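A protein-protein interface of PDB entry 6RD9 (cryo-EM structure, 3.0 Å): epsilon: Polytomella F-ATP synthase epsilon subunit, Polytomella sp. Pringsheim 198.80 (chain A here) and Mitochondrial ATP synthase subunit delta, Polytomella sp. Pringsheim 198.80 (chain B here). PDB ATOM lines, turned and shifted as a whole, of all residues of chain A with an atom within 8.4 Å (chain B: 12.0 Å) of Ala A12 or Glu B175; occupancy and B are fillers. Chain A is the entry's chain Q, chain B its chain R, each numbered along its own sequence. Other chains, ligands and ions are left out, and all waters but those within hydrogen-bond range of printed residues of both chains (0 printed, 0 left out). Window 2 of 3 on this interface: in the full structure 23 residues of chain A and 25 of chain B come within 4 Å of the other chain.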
ATOM      1  N   ALA A   3     -15.173 -38.793  26.329  1.00  0.00           N
ATOM      2  CA  ALA A   3     -14.472 -39.505  25.263  1.00  0.00           C
ATOM      3  C   ALA A   3     -13.520 -38.637  24.404  1.00  0.00           C
ATOM      4  O   ALA A   3     -12.498 -39.158  23.953  1.00  0.00           O
ATOM      5  CB  ALA A   3     -15.484 -40.242  24.371  1.00  0.00           C
ATOM      6  N   PRO A   4     -13.808 -37.355  24.152  1.00  0.00           N
ATOM      7  CA  PRO A   4     -12.724 -36.458  23.748  1.00  0.00           C
ATOM      8  C   PRO A   4     -12.014 -35.909  24.973  1.00  0.00           C
ATOM      9  O   PRO A   4     -12.537 -35.924  26.086  1.00  0.00           O
ATOM     10  CB  PRO A   4     -13.434 -35.338  22.974  1.00  0.00           C
ATOM     11  CG  PRO A   4     -14.784 -35.867  22.678  1.00  0.00           C
ATOM     12  CD  PRO A   4     -15.103 -36.704  23.866  1.00  0.00           C
ATOM     13  N   SER A   5     -10.801 -35.424  24.746  1.00  0.00           N
ATOM     14  CA  SER A   5      -9.949 -34.906  25.806  1.00  0.00           C
ATOM     15  C   SER A   5      -9.612 -33.458  25.496  1.00  0.00           C
ATOM     16  O   SER A   5      -9.106 -33.155  24.413  1.00  0.00           O
ATOM     17  CB  SER A   5      -8.678 -35.743  25.938  1.00  0.00           C
ATOM     18  OG  SER A   5      -7.875 -35.645  24.777  1.00  0.00           O
ATOM     19  N   GLY A   6      -9.892 -32.572  26.441  1.00  0.00           N
ATOM     20  CA  GLY A   6      -9.622 -31.169  26.264  1.00  0.00           C
ATOM     21  C   GLY A   6     -10.418 -30.298  27.205  1.00  0.00           C
ATOM     22  O   GLY A   6     -10.699 -30.673  28.346  1.00  0.00           O
ATOM     23  N   PRO A   7     -10.809 -29.117  26.740  1.00  0.00           N
ATOM     24  CA  PRO A   7     -11.581 -28.208  27.593  1.00  0.00           C
ATOM     25  C   PRO A   7     -13.004 -28.673  27.839  1.00  0.00           C
ATOM     26  O   PRO A   7     -13.419 -29.718  27.335  1.00  0.00           O
ATOM     27  CB  PRO A   7     -11.545 -26.888  26.816  1.00  0.00           C
ATOM     28  CG  PRO A   7     -10.433 -27.044  25.835  1.00  0.00           C
ATOM     29  CD  PRO A   7     -10.385 -28.470  25.491  1.00  0.00           C
ATOM     30  N   PHE A   8     -13.759 -27.900  28.621  1.00  0.00           N
ATOM     31  CA  PHE A   8     -15.055 -28.369  29.088  1.00  0.00           C
ATOM     32  C   PHE A   8     -16.096 -28.396  27.987  1.00  0.00           C
ATOM     33  O   PHE A   8     -17.087 -29.122  28.106  1.00  0.00           O
ATOM     34  CB  PHE A   8     -15.552 -27.515  30.252  1.00  0.00           C
ATOM     35  CG  PHE A   8     -15.796 -26.076  29.913  1.00  0.00           C
ATOM     36  CD1 PHE A   8     -17.068 -25.631  29.609  1.00  0.00           C
ATOM     37  CD2 PHE A   8     -14.764 -25.156  29.956  1.00  0.00           C
ATOM     38  CE1 PHE A   8     -17.296 -24.309  29.320  1.00  0.00           C
ATOM     39  CE2 PHE A   8     -14.986 -23.835  29.668  1.00  0.00           C
ATOM     40  CZ  PHE A   8     -16.253 -23.410  29.354  1.00  0.00           C
ATOM     41  N   TYR A   9     -15.901 -27.625  26.929  1.00  0.00           N
ATOM     42  CA  TYR A   9     -16.774 -27.723  25.774  1.00  0.00           C
ATOM     43  C   TYR A   9     -16.368 -28.876  24.875  1.00  0.00           C
ATOM     44  O   TYR A   9     -17.228 -29.547  24.304  1.00  0.00           O
ATOM     45  CB  TYR A   9     -16.769 -26.407  24.992  1.00  0.00           C
ATOM     46  CG  TYR A   9     -15.406 -25.820  24.727  1.00  0.00           C
ATOM     47  CD1 TYR A   9     -14.853 -24.891  25.589  1.00  0.00           C
ATOM     48  CD2 TYR A   9     -14.685 -26.174  23.600  1.00  0.00           C
ATOM     49  CE1 TYR A   9     -13.620 -24.353  25.346  1.00  0.00           C
ATOM     50  CE2 TYR A   9     -13.451 -25.643  23.355  1.00  0.00           C
ATOM     51  CZ  TYR A   9     -12.925 -24.735  24.228  1.00  0.00           C
ATOM     52  OH  TYR A   9     -11.692 -24.201  23.979  1.00  0.00           O
ATOM     53  N   ARG A  10     -15.069 -29.142  24.770  1.00  0.00           N
ATOM     54  CA  ARG A  10     -14.597 -30.141  23.824  1.00  0.00           C
ATOM     55  C   ARG A  10     -14.848 -31.555  24.322  1.00  0.00           C
ATOM     56  O   ARG A  10     -15.161 -32.441  23.521  1.00  0.00           O
ATOM     57  CB  ARG A  10     -13.118 -29.923  23.545  1.00  0.00           C
ATOM     58  CG  ARG A  10     -12.584 -30.713  22.396  1.00  0.00           C
ATOM     59  CD  ARG A  10     -13.200 -30.252  21.103  1.00  0.00           C
ATOM     60  NE  ARG A  10     -12.747 -28.922  20.718  1.00  0.00           N
ATOM     61  CZ  ARG A  10     -12.933 -28.406  19.510  1.00  0.00           C
ATOM     62  NH1 ARG A  10     -13.545 -29.118  18.579  1.00  0.00           N
ATOM     63  NH2 ARG A  10     -12.493 -27.193  19.224  1.00  0.00           N
ATOM     64  N   VAL A  11     -14.741 -31.787  25.634  1.00  0.00           N
ATOM     65  CA  VAL A  11     -15.071 -33.104  26.171  1.00  0.00           C
ATOM     66  C   VAL A  11     -16.573 -33.340  26.198  1.00  0.00           C
ATOM     67  O   VAL A  11     -17.008 -34.496  26.254  1.00  0.00           O
ATOM     68  CB  VAL A  11     -14.486 -33.322  27.579  1.00  0.00           C
ATOM     69  CG1 VAL A  11     -13.014 -33.032  27.585  1.00  0.00           C
ATOM     70  CG2 VAL A  11     -15.185 -32.459  28.615  1.00  0.00           C
ATOM     71  N   ALA A  12     -17.376 -32.283  26.132  1.00  0.00           N
ATOM     72  CA  ALA A  12     -18.821 -32.401  26.066  1.00  0.00           C
ATOM     73  C   ALA A  12     -19.330 -32.500  24.637  1.00  0.00           C
ATOM     74  O   ALA A  12     -20.524 -32.293  24.403  1.00  0.00           O
ATOM     75  CB  ALA A  12     -19.481 -31.219  26.775  1.00  0.00           C
ATOM     76  N   GLY A  13     -18.450 -32.786  23.676  1.00  0.00           N
ATOM     77  CA  GLY A  13     -18.821 -32.918  22.284  1.00  0.00           C
ATOM     78  C   GLY A  13     -18.981 -31.615  21.537  1.00  0.00           C
ATOM     79  O   GLY A  13     -19.039 -31.633  20.301  1.00  0.00           O
ATOM     80  N   MET A  14     -19.036 -30.490  22.239  1.00  0.00           N
ATOM     81  CA  MET A  14     -19.282 -29.202  21.615  1.00  0.00           C
ATOM     82  C   MET A  14     -18.015 -28.688  20.946  1.00  0.00           C
ATOM     83  O   MET A  14     -16.912 -28.851  21.468  1.00  0.00           O
ATOM     84  CB  MET A  14     -19.779 -28.217  22.669  1.00  0.00           C
ATOM     85  CG  MET A  14     -20.227 -26.893  22.141  1.00  0.00           C
ATOM     86  SD  MET A  14     -20.451 -25.688  23.448  1.00  0.00           S
ATOM     87  CE  MET A  14     -21.396 -26.606  24.629  1.00  0.00           C
ATOM     88  N   SER A  15     -18.171 -28.093  19.770  1.00  0.00           N
ATOM     89  CA  SER A  15     -17.058 -27.470  19.083  1.00  0.00           C
ATOM     90  C   SER A  15     -16.740 -26.125  19.724  1.00  0.00           C
ATOM     91  O   SER A  15     -17.518 -25.587  20.515  1.00  0.00           O
ATOM     92  CB  SER A  15     -17.383 -27.287  17.606  1.00  0.00           C
ATOM     93  OG  SER A  15     -18.291 -26.217  17.425  1.00  0.00           O
ATOM     94  N   LYS A  71     -28.315 -23.199  22.429  1.00  0.00           N
ATOM     95  CA  LYS A  71     -27.607 -23.557  23.648  1.00  0.00           C
ATOM     96  C   LYS A  71     -27.711 -25.035  23.973  1.00  0.00           C
ATOM     97  O   LYS A  71     -26.852 -25.561  24.687  1.00  0.00           O
ATOM     98  CB  LYS A  71     -28.157 -22.752  24.824  1.00  0.00           C
ATOM     99  CG  LYS A  71     -28.067 -21.256  24.654  1.00  0.00           C
ATOM    100  CD  LYS A  71     -29.041 -20.545  25.571  1.00  0.00           C
ATOM    101  CE  LYS A  71     -28.920 -19.042  25.427  1.00  0.00           C
ATOM    102  NZ  LYS A  71     -28.981 -18.592  24.014  1.00  0.00           N
ATOM    103  N   THR A  72     -28.730 -25.715  23.463  1.00  0.00           N
ATOM    104  CA  THR A  72     -28.951 -27.113  23.778  1.00  0.00           C
ATOM    105  C   THR A  72     -28.081 -28.004  22.897  1.00  0.00           C
ATOM    106  O   THR A  72     -27.221 -27.539  22.148  1.00  0.00           O
ATOM    107  CB  THR A  72     -30.427 -27.464  23.624  1.00  0.00           C
ATOM    108  OG1 THR A  72     -30.744 -27.590  22.232  1.00  0.00           O
ATOM    109  CG2 THR A  72     -31.285 -26.373  24.235  1.00  0.00           C
ATOM    110  N   ALA A  73     -28.312 -29.308  22.995  1.00  0.00           N
ATOM    111  CA  ALA A  73     -27.541 -30.273  22.226  1.00  0.00           C
ATOM    112  C   ALA A  73     -27.987 -30.279  20.771  1.00  0.00           C
ATOM    113  O   ALA A  73     -29.182 -30.201  20.475  1.00  0.00           O
ATOM    114  CB  ALA A  73     -27.694 -31.668  22.826  1.00  0.00           C
ATOM    115  N   ASN A  74     -27.023 -30.380  19.865  1.00  0.00           N
ATOM    116  CA  ASN A  74     -27.307 -30.419  18.436  1.00  0.00           C
ATOM    117  C   ASN A  74     -27.622 -31.838  17.970  1.00  0.00           C
ATOM    118  O   ASN A  74     -28.710 -32.112  17.460  1.00  0.00           O
ATOM    119  CB  ASN A  74     -26.124 -29.852  17.650  1.00  0.00           C
ATOM    120  CG  ASN A  74     -24.849 -30.645  17.863  1.00  0.00           C
ATOM    121  OD1 ASN A  74     -24.623 -31.207  18.935  1.00  0.00           O
ATOM    122  ND2 ASN A  74     -24.001 -30.682  16.845  1.00  0.00           N
ATOM    123  N   ALA B 170     -30.450 -23.774  37.050  1.00  0.00           N
ATOM    124  CA  ALA B 170     -30.845 -24.754  36.042  1.00  0.00           C
ATOM    125  C   ALA B 170     -29.621 -25.538  35.581  1.00  0.00           C
ATOM    126  O   ALA B 170     -28.957 -25.156  34.617  1.00  0.00           O
ATOM    127  CB  ALA B 170     -31.533 -24.060  34.872  1.00  0.00           C
ATOM    128  N   GLN B 171     -29.337 -26.649  36.255  1.00  0.00           N
ATOM    129  CA  GLN B 171     -28.287 -27.577  35.830  1.00  0.00           C
ATOM    130  C   GLN B 171     -28.872 -28.979  35.766  1.00  0.00           C
ATOM    131  O   GLN B 171     -28.886 -29.698  36.781  1.00  0.00           O
ATOM    132  CB  GLN B 171     -27.055 -27.563  36.734  1.00  0.00           C
ATOM    133  CG  GLN B 171     -26.328 -26.232  36.900  1.00  0.00           C
ATOM    134  CD  GLN B 171     -27.042 -25.265  37.804  1.00  0.00           C
ATOM    135  OE1 GLN B 171     -27.861 -25.665  38.631  1.00  0.00           O
ATOM    136  NE2 GLN B 171     -26.749 -23.985  37.645  1.00  0.00           N
ATOM    137  N   PRO B 172     -29.366 -29.400  34.609  1.00  0.00           N
ATOM    138  CA  PRO B 172     -29.842 -30.777  34.469  1.00  0.00           C
ATOM    139  C   PRO B 172     -28.711 -31.713  34.080  1.00  0.00           C
ATOM    140  O   PRO B 172     -27.550 -31.296  34.004  1.00  0.00           O
ATOM    141  CB  PRO B 172     -30.904 -30.673  33.368  1.00  0.00           C
ATOM    142  CG  PRO B 172     -30.593 -29.393  32.623  1.00  0.00           C
ATOM    143  CD  PRO B 172     -29.524 -28.636  33.363  1.00  0.00           C
ATOM    144  N   THR B 173     -29.038 -32.978  33.825  1.00  0.00           N
ATOM    145  CA  THR B 173     -28.040 -33.971  33.447  1.00  0.00           C
ATOM    146  C   THR B 173     -27.725 -33.932  31.946  1.00  0.00           C
ATOM    147  O   THR B 173     -27.086 -34.855  31.428  1.00  0.00           O
ATOM    148  CB  THR B 173     -28.527 -35.360  33.881  1.00  0.00           C
ATOM    149  OG1 THR B 173     -29.320 -35.220  35.066  1.00  0.00           O
ATOM    150  CG2 THR B 173     -27.348 -36.269  34.261  1.00  0.00           C
ATOM    151  N   ASP B 174     -28.157 -32.891  31.234  1.00  0.00           N
ATOM    152  CA  ASP B 174     -27.732 -32.685  29.855  1.00  0.00           C
ATOM    153  C   ASP B 174     -26.249 -32.329  29.833  1.00  0.00           C
ATOM    154  O   ASP B 174     -25.845 -31.285  30.356  1.00  0.00           O
ATOM    155  CB  ASP B 174     -28.566 -31.583  29.205  1.00  0.00           C
ATOM    156  CG  ASP B 174     -28.469 -31.593  27.689  1.00  0.00           C
ATOM    157  OD1 ASP B 174     -29.126 -30.749  27.046  1.00  0.00           O
ATOM    158  OD2 ASP B 174     -27.751 -32.449  27.137  1.00  0.00           O
ATOM    159  N   GLU B 175     -25.436 -33.203  29.238  1.00  0.00           N
ATOM    160  CA  GLU B 175     -23.991 -33.004  29.268  1.00  0.00           C
ATOM    161  C   GLU B 175     -23.558 -31.944  28.261  1.00  0.00           C
ATOM    162  O   GLU B 175     -22.441 -31.427  28.334  1.00  0.00           O
ATOM    163  CB  GLU B 175     -23.274 -34.334  29.034  1.00  0.00           C
ATOM    164  CG  GLU B 175     -23.468 -34.956  27.665  1.00  0.00           C
ATOM    165  CD  GLU B 175     -22.324 -34.636  26.735  1.00  0.00           C
ATOM    166  OE1 GLU B 175     -21.241 -34.305  27.257  1.00  0.00           O
ATOM    167  OE2 GLU B 175     -22.498 -34.711  25.500  1.00  0.00           O
ATOM    168  N   PHE B 176     -24.408 -31.646  27.284  1.00  0.00           N
ATOM    169  CA  PHE B 176     -24.159 -30.499  26.422  1.00  0.00           C
ATOM    170  C   PHE B 176     -24.480 -29.198  27.145  1.00  0.00           C
ATOM    171  O   PHE B 176     -23.780 -28.194  26.979  1.00  0.00           O
ATOM    172  CB  PHE B 176     -24.983 -30.625  25.152  1.00  0.00           C
ATOM    173  CG  PHE B 176     -24.380 -29.949  23.969  1.00  0.00           C
ATOM    174  CD1 PHE B 176     -23.622 -30.669  23.064  1.00  0.00           C
ATOM    175  CD2 PHE B 176     -24.592 -28.601  23.741  1.00  0.00           C
ATOM    176  CE1 PHE B 176     -23.078 -30.058  21.958  1.00  0.00           C
ATOM    177  CE2 PHE B 176     -24.053 -27.984  22.641  1.00  0.00           C
ATOM    178  CZ  PHE B 176     -23.295 -28.714  21.750  1.00  0.00           C
ATOM    179  N   GLU B 177     -25.539 -29.192  27.951  1.00  0.00           N
ATOM    180  CA  GLU B 177     -25.809 -28.047  28.804  1.00  0.00           C
ATOM    181  C   GLU B 177     -24.946 -28.056  30.056  1.00  0.00           C
ATOM    182  O   GLU B 177     -24.991 -27.093  30.822  1.00  0.00           O
ATOM    183  CB  GLU B 177     -27.291 -28.001  29.184  1.00  0.00           C
ATOM    184  CG  GLU B 177     -27.918 -26.606  29.179  1.00  0.00           C
ATOM    185  CD  GLU B 177     -27.845 -25.898  30.518  1.00  0.00           C
ATOM    186  OE1 GLU B 177     -27.759 -26.581  31.554  1.00  0.00           O
ATOM    187  OE2 GLU B 177     -27.883 -24.654  30.539  1.00  0.00           O
ATOM    188  N   GLN B 178     -24.182 -29.127  30.292  1.00  0.00           N
ATOM    189  CA  GLN B 178     -23.138 -29.092  31.309  1.00  0.00           C
ATOM    190  C   GLN B 178     -22.098 -28.036  30.968  1.00  0.00           C
ATOM    191  O   GLN B 178     -21.651 -27.278  31.836  1.00  0.00           O
ATOM    192  CB  GLN B 178     -22.474 -30.465  31.438  1.00  0.00           C
ATOM    193  CG  GLN B 178     -21.385 -30.548  32.493  1.00  0.00           C
ATOM    194  CD  GLN B 178     -21.934 -30.393  33.886  1.00  0.00           C
ATOM    195  OE1 GLN B 178     -21.868 -29.317  34.479  1.00  0.00           O
ATOM    196  NE2 GLN B 178     -22.465 -31.480  34.431  1.00  0.00           N
ATOM    197  N   ALA B 179     -21.709 -27.967  29.697  1.00  0.00           N
ATOM    198  CA  ALA B 179     -20.731 -26.972  29.280  1.00  0.00           C
ATOM    199  C   ALA B 179     -21.380 -25.612  29.061  1.00  0.00           C
ATOM    200  O   ALA B 179     -20.798 -24.580  29.414  1.00  0.00           O
ATOM    201  CB  ALA B 179     -20.021 -27.447  28.013  1.00  0.00           C
ATOM    202  N   ALA B 180     -22.592 -25.592  28.498  1.00  0.00           N
ATOM    203  CA  ALA B 180     -23.226 -24.328  28.130  1.00  0.00           C
ATOM    204  C   ALA B 180     -23.702 -23.563  29.354  1.00  0.00           C
ATOM    205  O   ALA B 180     -23.778 -22.331  29.332  1.00  0.00           O
ATOM    206  CB  ALA B 180     -24.391 -24.576  27.176  1.00  0.00           C
ATOM    207  N   ASN B 181     -24.045 -24.271  30.425  1.00  0.00           N
ATOM    208  CA  ASN B 181     -24.342 -23.557  31.654  1.00  0.00           C
ATOM    209  C   ASN B 181     -23.056 -23.142  32.351  1.00  0.00           C
ATOM    210  O   ASN B 181     -23.011 -22.076  32.974  1.00  0.00           O
ATOM    211  CB  ASN B 181     -25.201 -24.418  32.570  1.00  0.00           C
ATOM    212  CG  ASN B 181     -25.978 -23.608  33.568  1.00  0.00           C
ATOM    213  OD1 ASN B 181     -25.440 -22.760  34.264  1.00  0.00           O
ATOM    214  ND2 ASN B 181     -27.270 -23.871  33.641  1.00  0.00           N
ATOM    215  N   ARG B 182     -22.002 -23.958  32.238  1.00  0.00           N
ATOM    216  CA  ARG B 182     -20.698 -23.577  32.775  1.00  0.00           C
ATOM    217  C   ARG B 182     -20.174 -22.326  32.086  1.00  0.00           C
ATOM    218  O   ARG B 182     -19.649 -21.416  32.739  1.00  0.00           O
ATOM    219  CB  ARG B 182     -19.705 -24.729  32.617  1.00  0.00           C
ATOM    220  CG  ARG B 182     -18.267 -24.354  32.930  1.00  0.00           C
ATOM    221  CD  ARG B 182     -17.415 -25.570  33.209  1.00  0.00           C
ATOM    222  NE  ARG B 182     -15.995 -25.237  33.255  1.00  0.00           N
ATOM    223  CZ  ARG B 182     -15.032 -26.118  33.496  1.00  0.00           C
ATOM    224  NH1 ARG B 182     -15.336 -27.386  33.709  1.00  0.00           N
ATOM    225  NH2 ARG B 182     -13.767 -25.733  33.519  1.00  0.00           N
ATOM    226  N   ALA B 183     -20.355 -22.249  30.767  1.00  0.00           N
ATOM    227  CA  ALA B 183     -20.000 -21.043  30.033  1.00  0.00           C
ATOM    228  C   ALA B 183     -20.918 -19.887  30.395  1.00  0.00           C
ATOM    229  O   ALA B 183     -20.507 -18.723  30.354  1.00  0.00           O
ATOM    230  CB  ALA B 183     -20.053 -21.319  28.537  1.00  0.00           C
ATOM    231  N   ALA B 184     -22.162 -20.190  30.764  1.00  0.00           N
ATOM    232  CA  ALA B 184     -23.089 -19.145  31.177  1.00  0.00           C
ATOM    233  C   ALA B 184     -22.699 -18.570  32.529  1.00  0.00           C
ATOM    234  O   ALA B 184     -22.817 -17.362  32.760  1.00  0.00           O
ATOM    235  CB  ALA B 184     -24.512 -19.692  31.222  1.00  0.00           C
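Of the 17 printed residues of chain A, 8 touch a printed residue of chain B.
Hydrophobic or aromatic side chains of chain A that line the printed part of chain B: Phe A8, Ala A12, Met A14 and Ala A73.
Printed residues of chain B that touch a printed residue of chain A: Glu B175, Phe B176, Ala B179, Ala B180, Arg B182 and Ala B183.
Among the printed residues, no Asp or Glu carboxylate lies within 4 Å of a Lys or Arg side-chain nitrogen of the other chain.
Among the printed residues, merely in contact across the chains: Phe A8 with Ala B179, Phe A8 with Arg B182, Phe A8 with Ala B183, Tyr A9 with Ala B179, Ala A12 with Phe B176, Met A14 with Phe B176, Met A14 with Ala B179, Lys A71 with Phe B176, Lys A71 with Ala B180, Thr A72 with Phe B176, Ala A73 with Phe B176 and Asn A74 with Phe B176.
The backbone carbonyl oxygen (O) of Tyr A9 sits at hydrogen-bond distance from the backbone NH (N) of Met A14 (2.9 Å).
N of Phe B176 lies close to OD2 of Asp B174, at 3.4 Å.
OE2 of Glu B175 sits close to O of Ala A12 (3.3 Å).
No residue of chain B comes within 4 Å of Gly A6.
No residue of chain B comes within 4 Å of Val A11.
Of the printed residues of chain B, Ala A12 touches Glu B175 and Phe B176.
No residue of chain B comes within 4 Å of Gly A13.
Printed residues of chain B within 4 Å of Met A14: Phe B176 (3.6 Å) and Ala B179 (3.7 Å).
Of the printed residues of chain B, Thr A72 touches Phe B176.
Of the printed residues of chain A, Phe B176 touches Ala A12, Met A14, Lys A71, Thr A72, Ala A73 and Asn A74.
Ala B184 touches none of the printed residues of chain A.
The nearest residue of chain A that does not touch Glu B175 is Val A11 (4.4 Å).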
